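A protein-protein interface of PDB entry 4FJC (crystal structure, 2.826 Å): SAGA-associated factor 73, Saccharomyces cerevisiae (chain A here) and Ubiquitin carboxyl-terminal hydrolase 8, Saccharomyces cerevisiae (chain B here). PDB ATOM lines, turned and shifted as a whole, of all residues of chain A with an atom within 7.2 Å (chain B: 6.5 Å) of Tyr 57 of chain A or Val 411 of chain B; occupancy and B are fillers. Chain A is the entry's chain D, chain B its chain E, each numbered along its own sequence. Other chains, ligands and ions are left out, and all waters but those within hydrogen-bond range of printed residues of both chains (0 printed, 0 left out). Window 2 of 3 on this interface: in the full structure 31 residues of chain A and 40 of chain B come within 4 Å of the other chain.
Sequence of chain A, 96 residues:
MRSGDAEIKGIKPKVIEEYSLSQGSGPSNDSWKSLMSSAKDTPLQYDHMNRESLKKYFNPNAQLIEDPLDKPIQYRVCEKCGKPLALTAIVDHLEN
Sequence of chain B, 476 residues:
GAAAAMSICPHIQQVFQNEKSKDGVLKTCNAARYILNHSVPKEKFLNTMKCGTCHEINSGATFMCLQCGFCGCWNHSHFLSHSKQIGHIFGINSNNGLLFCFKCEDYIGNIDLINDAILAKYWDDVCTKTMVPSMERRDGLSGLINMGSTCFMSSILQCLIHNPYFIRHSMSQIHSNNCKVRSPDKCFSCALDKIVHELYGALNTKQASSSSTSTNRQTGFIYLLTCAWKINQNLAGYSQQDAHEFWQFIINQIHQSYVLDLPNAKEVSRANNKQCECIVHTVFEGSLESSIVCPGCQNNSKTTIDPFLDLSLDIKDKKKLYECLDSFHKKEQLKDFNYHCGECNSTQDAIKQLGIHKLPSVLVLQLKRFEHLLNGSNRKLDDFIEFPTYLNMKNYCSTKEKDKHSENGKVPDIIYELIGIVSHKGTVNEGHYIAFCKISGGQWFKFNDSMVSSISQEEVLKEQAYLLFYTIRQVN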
ATOM      1  N   GLU A  52       0.820  -0.099  29.145  1.00  0.00           N
ATOM      2  CA  GLU A  52       0.254  -0.889  30.224  1.00  0.00           C
ATOM      3  C   GLU A  52       0.625  -2.334  30.047  1.00  0.00           C
ATOM      4  O   GLU A  52       0.965  -3.007  31.020  1.00  0.00           O
ATOM      5  CB  GLU A  52      -1.271  -0.741  30.333  1.00  0.00           C
ATOM      6  CG  GLU A  52      -1.759   0.650  30.769  1.00  0.00           C
ATOM      7  CD  GLU A  52      -1.881   1.677  29.613  1.00  0.00           C
ATOM      8  OE1 GLU A  52      -1.327   2.797  29.763  1.00  0.00           O
ATOM      9  OE2 GLU A  52      -2.521   1.384  28.552  1.00  0.00           O
ATOM     10  N   SER A  53       0.580  -2.824  28.813  1.00  0.00           N
ATOM     11  CA  SER A  53       1.009  -4.209  28.552  1.00  0.00           C
ATOM     12  C   SER A  53       2.474  -4.391  28.937  1.00  0.00           C
ATOM     13  O   SER A  53       2.830  -5.425  29.496  1.00  0.00           O
ATOM     14  CB  SER A  53       0.804  -4.609  27.091  1.00  0.00           C
ATOM     15  OG  SER A  53      -0.563  -4.852  26.799  1.00  0.00           O
ATOM     16  N   LEU A  54       3.297  -3.375  28.662  1.00  0.00           N
ATOM     17  CA  LEU A  54       4.726  -3.391  29.014  1.00  0.00           C
ATOM     18  C   LEU A  54       4.998  -3.554  30.508  1.00  0.00           C
ATOM     19  O   LEU A  54       5.808  -4.386  30.892  1.00  0.00           O
ATOM     20  CB  LEU A  54       5.435  -2.126  28.513  1.00  0.00           C
ATOM     21  CG  LEU A  54       5.849  -2.032  27.033  1.00  0.00           C
ATOM     22  CD1 LEU A  54       6.532  -0.696  26.764  1.00  0.00           C
ATOM     23  CD2 LEU A  54       6.751  -3.194  26.632  1.00  0.00           C
ATOM     24  N   LYS A  55       4.356  -2.761  31.355  1.00  0.00           N
ATOM     25  CA  LYS A  55       4.428  -3.009  32.802  1.00  0.00           C
ATOM     26  C   LYS A  55       4.106  -4.485  33.140  1.00  0.00           C
ATOM     27  O   LYS A  55       4.894  -5.152  33.807  1.00  0.00           O
ATOM     28  CB  LYS A  55       3.478  -2.077  33.584  1.00  0.00           C
ATOM     29  CG  LYS A  55       3.840  -0.589  33.533  1.00  0.00           C
ATOM     30  CD  LYS A  55       3.244   0.208  34.708  1.00  0.00           C
ATOM     31  CE  LYS A  55       1.939   0.961  34.386  1.00  0.00           C
ATOM     32  NZ  LYS A  55       2.082   2.184  33.509  1.00  0.00           N
ATOM     33  N   LYS A  56       2.963  -4.984  32.651  1.00  0.00           N
ATOM     34  CA  LYS A  56       2.471  -6.338  32.961  1.00  0.00           C
ATOM     35  C   LYS A  56       3.383  -7.476  32.527  1.00  0.00           C
ATOM     36  O   LYS A  56       3.640  -8.379  33.305  1.00  0.00           O
ATOM     37  CB  LYS A  56       1.109  -6.595  32.303  1.00  0.00           C
ATOM     38  CG  LYS A  56      -0.057  -5.793  32.851  1.00  0.00           C
ATOM     39  CD  LYS A  56      -1.368  -6.246  32.234  1.00  0.00           C
ATOM     40  CE  LYS A  56      -2.589  -5.624  32.909  1.00  0.00           C
ATOM     41  NZ  LYS A  56      -3.192  -4.487  32.156  1.00  0.00           N
ATOM     42  N   TYR A  57       3.847  -7.451  31.282  1.00  0.00           N
ATOM     43  CA  TYR A  57       4.508  -8.625  30.696  1.00  0.00           C
ATOM     44  C   TYR A  57       6.027  -8.534  30.629  1.00  0.00           C
ATOM     45  O   TYR A  57       6.696  -9.551  30.506  1.00  0.00           O
ATOM     46  CB  TYR A  57       3.923  -8.910  29.324  1.00  0.00           C
ATOM     47  CG  TYR A  57       2.430  -9.119  29.412  1.00  0.00           C
ATOM     48  CD1 TYR A  57       1.900 -10.203  30.119  1.00  0.00           C
ATOM     49  CD2 TYR A  57       1.540  -8.218  28.830  1.00  0.00           C
ATOM     50  CE1 TYR A  57       0.532 -10.396  30.227  1.00  0.00           C
ATOM     51  CE2 TYR A  57       0.176  -8.411  28.921  1.00  0.00           C
ATOM     52  CZ  TYR A  57      -0.321  -9.495  29.624  1.00  0.00           C
ATOM     53  OH  TYR A  57      -1.683  -9.676  29.711  1.00  0.00           O
ATOM     54  N   PHE A  58       6.554  -7.320  30.738  1.00  0.00           N
ATOM     55  CA  PHE A  58       7.977  -7.071  30.730  1.00  0.00           C
ATOM     56  C   PHE A  58       8.435  -6.572  32.116  1.00  0.00           C
ATOM     57  O   PHE A  58       7.604  -6.226  32.969  1.00  0.00           O
ATOM     58  CB  PHE A  58       8.305  -6.045  29.627  1.00  0.00           C
ATOM     59  CG  PHE A  58       8.024  -6.550  28.245  1.00  0.00           C
ATOM     60  CD1 PHE A  58       6.733  -6.675  27.791  1.00  0.00           C
ATOM     61  CD2 PHE A  58       9.036  -6.938  27.426  1.00  0.00           C
ATOM     62  CE1 PHE A  58       6.459  -7.168  26.539  1.00  0.00           C
ATOM     63  CE2 PHE A  58       8.775  -7.432  26.176  1.00  0.00           C
ATOM     64  CZ  PHE A  58       7.481  -7.540  25.730  1.00  0.00           C
ATOM     65  N   ASN A  59       9.754  -6.546  32.338  1.00  0.00           N
ATOM     66  CA  ASN A  59      10.322  -6.121  33.622  1.00  0.00           C
ATOM     67  C   ASN A  59      10.325  -4.607  33.790  1.00  0.00           C
ATOM     68  O   ASN A  59      10.632  -3.886  32.853  1.00  0.00           O
ATOM     69  CB  ASN A  59      11.747  -6.617  33.766  1.00  0.00           C
ATOM     70  CG  ASN A  59      11.847  -8.116  33.669  1.00  0.00           C
ATOM     71  OD1 ASN A  59      11.638  -8.849  34.654  1.00  0.00           O
ATOM     72  ND2 ASN A  59      12.161  -8.594  32.469  1.00  0.00           N
ATOM     73  N   ILE B 356       5.370 -18.020  30.860  1.00  0.00           N
ATOM     74  CA  ILE B 356       6.295 -16.887  31.077  1.00  0.00           C
ATOM     75  C   ILE B 356       5.687 -15.776  31.935  1.00  0.00           C
ATOM     76  O   ILE B 356       4.655 -15.226  31.591  1.00  0.00           O
ATOM     77  CB  ILE B 356       6.798 -16.260  29.748  1.00  0.00           C
ATOM     78  CG1 ILE B 356       7.501 -17.301  28.876  1.00  0.00           C
ATOM     79  CG2 ILE B 356       7.741 -15.090  30.038  1.00  0.00           C
ATOM     80  CD1 ILE B 356       6.774 -17.605  27.603  1.00  0.00           C
ATOM     81  N   HIS B 357       6.351 -15.447  33.037  1.00  0.00           N
ATOM     82  CA  HIS B 357       5.933 -14.338  33.897  1.00  0.00           C
ATOM     83  C   HIS B 357       6.313 -13.007  33.303  1.00  0.00           C
ATOM     84  O   HIS B 357       5.488 -12.100  33.254  1.00  0.00           O
ATOM     85  CB  HIS B 357       6.552 -14.495  35.276  1.00  0.00           C
ATOM     86  CG  HIS B 357       6.040 -13.512  36.323  1.00  0.00           C
ATOM     87  ND1 HIS B 357       6.874 -12.714  37.039  1.00  0.00           N
ATOM     88  CD2 HIS B 357       4.757 -13.268  36.813  1.00  0.00           C
ATOM     89  CE1 HIS B 357       6.156 -11.981  37.920  1.00  0.00           C
ATOM     90  NE2 HIS B 357       4.865 -12.313  37.782  1.00  0.00           N
ATOM     91  N   LYS B 358       7.581 -12.892  32.878  1.00  0.00           N
ATOM     92  CA  LYS B 358       8.153 -11.686  32.246  1.00  0.00           C
ATOM     93  C   LYS B 358       8.946 -12.062  31.007  1.00  0.00           C
ATOM     94  O   LYS B 358       9.765 -12.973  31.040  1.00  0.00           O
ATOM     95  CB  LYS B 358       9.120 -10.951  33.171  1.00  0.00           C
ATOM     96  CG  LYS B 358       8.519 -10.374  34.425  1.00  0.00           C
ATOM     97  CD  LYS B 358       7.417  -9.381  34.110  1.00  0.00           C
ATOM     98  CE  LYS B 358       7.056  -8.530  35.316  1.00  0.00           C
ATOM     99  NZ  LYS B 358       5.991  -7.554  34.961  1.00  0.00           N
ATOM    100  N   LEU B 359       8.722 -11.320  29.931  1.00  0.00           N
ATOM    101  CA  LEU B 359       9.479 -11.470  28.706  1.00  0.00           C
ATOM    102  C   LEU B 359      10.695 -10.541  28.653  1.00  0.00           C
ATOM    103  O   LEU B 359      10.685  -9.414  29.142  1.00  0.00           O
ATOM    104  CB  LEU B 359       8.589 -11.170  27.510  1.00  0.00           C
ATOM    105  CG  LEU B 359       7.515 -12.229  27.266  1.00  0.00           C
ATOM    106  CD1 LEU B 359       6.202 -11.553  26.897  1.00  0.00           C
ATOM    107  CD2 LEU B 359       7.986 -13.233  26.217  1.00  0.00           C
ATOM    108  N   PRO B 360      11.759 -11.028  28.041  1.00  0.00           N
ATOM    109  CA  PRO B 360      12.883 -10.219  27.799  1.00  0.00           C
ATOM    110  C   PRO B 360      12.642  -9.352  26.567  1.00  0.00           C
ATOM    111  O   PRO B 360      11.642  -9.500  25.875  1.00  0.00           O
ATOM    112  CB  PRO B 360      13.943 -11.254  27.508  1.00  0.00           C
ATOM    113  CG  PRO B 360      13.200 -12.250  26.682  1.00  0.00           C
ATOM    114  CD  PRO B 360      11.872 -12.328  27.361  1.00  0.00           C
ATOM    115  N   MET B 393       4.039 -14.080  20.879  1.00  0.00           N
ATOM    116  CA  MET B 393       4.315 -14.804  22.128  1.00  0.00           C
ATOM    117  C   MET B 393       3.184 -14.741  23.121  1.00  0.00           C
ATOM    118  O   MET B 393       3.312 -15.260  24.219  1.00  0.00           O
ATOM    119  CB  MET B 393       5.586 -14.279  22.817  1.00  0.00           C
ATOM    120  CG  MET B 393       6.888 -14.660  22.148  1.00  0.00           C
ATOM    121  SD  MET B 393       7.171 -16.430  21.991  1.00  0.00           S
ATOM    122  CE  MET B 393       7.932 -16.875  23.555  1.00  0.00           C
ATOM    123  N   LYS B 394       2.069 -14.132  22.754  1.00  0.00           N
ATOM    124  CA  LYS B 394       0.949 -13.985  23.703  1.00  0.00           C
ATOM    125  C   LYS B 394       0.457 -15.315  24.281  1.00  0.00           C
ATOM    126  O   LYS B 394       0.008 -15.389  25.430  1.00  0.00           O
ATOM    127  CB  LYS B 394      -0.215 -13.280  23.036  1.00  0.00           C
ATOM    128  CG  LYS B 394      -0.851 -14.063  21.909  1.00  0.00           C
ATOM    129  CD  LYS B 394      -1.818 -13.187  21.153  1.00  0.00           C
ATOM    130  CE  LYS B 394      -2.443 -13.894  19.976  1.00  0.00           C
ATOM    131  NZ  LYS B 394      -3.672 -13.130  19.653  1.00  0.00           N
ATOM    132  N   ASN B 395       0.528 -16.370  23.492  1.00  0.00           N
ATOM    133  CA  ASN B 395      -0.048 -17.621  23.944  1.00  0.00           C
ATOM    134  C   ASN B 395       0.765 -18.337  25.030  1.00  0.00           C
ATOM    135  O   ASN B 395       0.271 -19.293  25.629  1.00  0.00           O
ATOM    136  CB  ASN B 395      -0.260 -18.558  22.751  1.00  0.00           C
ATOM    137  CG  ASN B 395      -1.447 -18.167  21.909  1.00  0.00           C
ATOM    138  OD1 ASN B 395      -1.581 -18.609  20.769  1.00  0.00           O
ATOM    139  ND2 ASN B 395      -2.320 -17.342  22.469  1.00  0.00           N
ATOM    140  N   CYS B 397       2.340 -16.622  27.710  1.00  0.00           N
ATOM    141  CA  CYS B 397       2.372 -15.846  28.945  1.00  0.00           C
ATOM    142  C   CYS B 397       1.155 -16.073  29.800  1.00  0.00           C
ATOM    143  O   CYS B 397       0.057 -16.266  29.291  1.00  0.00           O
ATOM    144  CB  CYS B 397       2.396 -14.363  28.655  1.00  0.00           C
ATOM    145  SG  CYS B 397       3.729 -13.838  27.602  1.00  0.00           S
ATOM    146  N   SER B 398       1.366 -15.940  31.103  1.00  0.00           N
ATOM    147  CA  SER B 398       0.345 -16.102  32.148  1.00  0.00           C
ATOM    148  C   SER B 398      -0.756 -15.011  32.169  1.00  0.00           C
ATOM    149  O   SER B 398      -0.598 -13.977  31.546  1.00  0.00           O
ATOM    150  CB  SER B 398       1.079 -16.108  33.491  1.00  0.00           C
ATOM    151  OG  SER B 398       2.346 -16.738  33.364  1.00  0.00           O
ATOM    152  N   THR B 399      -1.847 -15.234  32.907  1.00  0.00           N
ATOM    153  CA  THR B 399      -2.985 -14.283  32.971  1.00  0.00           C
ATOM    154  C   THR B 399      -3.716 -14.250  31.630  1.00  0.00           C
ATOM    155  O   THR B 399      -3.919 -15.299  31.013  1.00  0.00           O
ATOM    156  CB  THR B 399      -2.576 -12.835  33.416  1.00  0.00           C
ATOM    157  OG1 THR B 399      -2.387 -12.794  34.841  1.00  0.00           O
ATOM    158  CG2 THR B 399      -3.644 -11.764  33.001  1.00  0.00           C
ATOM    159  N   LYS B 410      -7.618 -11.882  28.259  1.00  0.00           N
ATOM    160  CA  LYS B 410      -6.533 -12.517  27.478  1.00  0.00           C
ATOM    161  C   LYS B 410      -5.399 -11.518  27.036  1.00  0.00           C
ATOM    162  O   LYS B 410      -5.652 -10.320  26.762  1.00  0.00           O
ATOM    163  CB  LYS B 410      -7.105 -13.249  26.240  1.00  0.00           C
ATOM    164  CG  LYS B 410      -7.122 -12.388  24.992  1.00  0.00           C
ATOM    165  CD  LYS B 410      -8.249 -12.674  24.018  1.00  0.00           C
ATOM    166  CE  LYS B 410      -8.616 -11.404  23.232  1.00  0.00           C
ATOM    167  NZ  LYS B 410      -9.803 -11.572  22.352  1.00  0.00           N
ATOM    168  N   VAL B 411      -4.171 -12.052  26.953  1.00  0.00           N
ATOM    169  CA  VAL B 411      -2.942 -11.298  26.666  1.00  0.00           C
ATOM    170  C   VAL B 411      -3.002 -10.728  25.272  1.00  0.00           C
ATOM    171  O   VAL B 411      -3.454 -11.411  24.370  1.00  0.00           O
ATOM    172  CB  VAL B 411      -1.735 -12.251  26.684  1.00  0.00           C
ATOM    173  CG1 VAL B 411      -0.441 -11.482  26.482  1.00  0.00           C
ATOM    174  CG2 VAL B 411      -1.707 -13.079  27.968  1.00  0.00           C
ATOM    175  N   PRO B 412      -2.534  -9.490  25.068  1.00  0.00           N
ATOM    176  CA  PRO B 412      -2.611  -8.962  23.688  1.00  0.00           C
ATOM    177  C   PRO B 412      -1.529  -9.541  22.779  1.00  0.00           C
ATOM    178  O   PRO B 412      -0.832 -10.445  23.156  1.00  0.00           O
ATOM    179  CB  PRO B 412      -2.437  -7.453  23.860  1.00  0.00           C
ATOM    180  CG  PRO B 412      -1.838  -7.255  25.214  1.00  0.00           C
ATOM    181  CD  PRO B 412      -1.858  -8.558  25.986  1.00  0.00           C
ATOM    182  N   ASP B 413      -1.411  -9.033  21.575  1.00  0.00           N
ATOM    183  CA  ASP B 413      -0.320  -9.424  20.710  1.00  0.00           C
ATOM    184  C   ASP B 413       1.014  -8.933  21.267  1.00  0.00           C
ATOM    185  O   ASP B 413       1.135  -7.784  21.697  1.00  0.00           O
ATOM    186  CB  ASP B 413      -0.530  -8.862  19.296  1.00  0.00           C
ATOM    187  CG  ASP B 413      -1.688  -9.524  18.579  1.00  0.00           C
ATOM    188  OD1 ASP B 413      -1.618 -10.743  18.348  1.00  0.00           O
ATOM    189  OD2 ASP B 413      -2.674  -8.821  18.253  1.00  0.00           O
ATOM    190  N   ILE B 414       1.995  -9.832  21.254  1.00  0.00           N
ATOM    191  CA  ILE B 414       3.374  -9.524  21.583  1.00  0.00           C
ATOM    192  C   ILE B 414       4.219 -10.225  20.529  1.00  0.00           C
ATOM    193  O   ILE B 414       4.283 -11.448  20.509  1.00  0.00           O
ATOM    194  CB  ILE B 414       3.764 -10.016  22.981  1.00  0.00           C
ATOM    195  CG1 ILE B 414       2.679  -9.597  24.008  1.00  0.00           C
ATOM    196  CG2 ILE B 414       5.143  -9.498  23.333  1.00  0.00           C
ATOM    197  CD1 ILE B 414       2.987  -9.908  25.467  1.00  0.00           C
ATOM    198  N   VAL B 475       4.026  -4.611  20.961  1.00  0.00           N
ATOM    199  CA  VAL B 475       3.127  -5.101  21.971  1.00  0.00           C
ATOM    200  C   VAL B 475       1.881  -4.237  22.035  1.00  0.00           C
ATOM    201  O   VAL B 475       1.962  -3.012  22.224  1.00  0.00           O
ATOM    202  CB  VAL B 475       3.791  -5.285  23.360  1.00  0.00           C
ATOM    203  CG1 VAL B 475       5.171  -4.673  23.403  1.00  0.00           C
ATOM    204  CG2 VAL B 475       2.904  -4.772  24.474  1.00  0.00           C
ATOM    205  N   ASN B 476       0.740  -4.903  21.840  1.00  0.00           N
ATOM    206  CA  ASN B 476      -0.574  -4.291  21.938  1.00  0.00           C
ATOM    207  C   ASN B 476      -1.137  -4.421  23.368  1.00  0.00           C
ATOM    208  O   ASN B 476      -0.377  -4.521  24.327  1.00  0.00           O
ATOM    209  CB  ASN B 476      -1.521  -4.931  20.914  1.00  0.00           C
ATOM    210  CG  ASN B 476      -1.226  -4.493  19.483  1.00  0.00           C
ATOM    211  OD1 ASN B 476      -0.538  -3.522  19.242  1.00  0.00           O
ATOM    212  ND2 ASN B 476      -1.777  -5.206  18.535  1.00  0.00           N
ATOM    213  OXT ASN B 476      -2.335  -4.415  23.660  1.00  0.00           O
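Hydrophobic or aromatic side chains of chain A within 4 Å of the printed part of chain B: Leu 54, Tyr 57 and Phe 58. Among the printed residues, no Asp or Glu carboxylate lies within 4 Å of a Lys or Arg side-chain nitrogen of the other chain.
Among the printed residues, pairs that only touch across the chains: Tyr 57 of chain A with Lys 358 of chain B (3.1 Å), Ser 53 of chain A with Pro 412 of chain B (3.1 Å), Ser 53 of chain A with Val 475 of chain B (3.4 Å), Phe 58 of chain A with Leu 359 of chain B (3.4 Å), Asn 59 of chain A with Lys 358 of chain B (3.5 Å), Phe 58 of chain A with Pro 360 of chain B (3.5 Å), Tyr 57 of chain A with Pro 412 of chain B (3.6 Å), Tyr 57 of chain A with Val 411 of chain B (3.7 Å), Asn 59 of chain A with Leu 359 of chain B (3.7 Å), Phe 58 of chain A with Ile 414 of chain B (3.9 Å), Leu 54 of chain A with Val 475 of chain B (3.9 Å), Tyr 57 of chain A with His 357 of chain B (3.9 Å) and Tyr 57 of chain A with Ser 398 of chain B (3.98 Å).
Printed residues of chain B within 4 Å of Ser 53 of chain A: Pro 412 (3.1 Å), Val 475 (3.4 Å) and Asn 476 (2.5 Å). Printed residues of chain B within 4 Å of Lys 55 of chain A: Lys 358 (2.9 Å). Of chain B, only His 357, Lys 358, Leu 359, Ser 398, Val 411 and Pro 412 come within 4 Å of Tyr 57 of chain A. Of the printed residues of chain A, Pro 360 of chain B touches Phe 58 (3.5 Å). Of the printed residues of chain A, Pro 412 of chain B touches Ser 53 and Tyr 57. The nearest residue of chain B that does not touch Tyr 57 of chain A is Ile 414 of chain B (4.03 Å).
The backbone carbonyl oxygen (O) of Asp 413 of chain B sits at hydrogen-bond distance from the backbone NH (N) of Asn 476 of chain B. N of Met 393 of chain B lies within hydrogen-bond range of O of Ile 414 of chain B (2.7 Å). O of Ile 356 of chain B is in hydrogen-bond range of OG of Ser 398 of chain B.
O of Tyr 57 of chain A lies within hydrogen-bond range of N of Leu 359 of chain B, at 2.8 Å. O of Phe 58 of chain A lies within hydrogen-bond range of NZ of Lys 358 of chain B, at 2.9 Å. The side-chain amino group (NZ) of Lys 358 of chain B is in hydrogen-bond range of the backbone carbonyl oxygen (O) of Lys 55 of chain A. NZ of Lys 358 of chain B is in hydrogen-bond range of O of Lys 56 of chain A (3.0 Å). O of Asn 476 of chain B is in hydrogen-bond range of OG of Ser 53 of chain A (2.5 Å).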
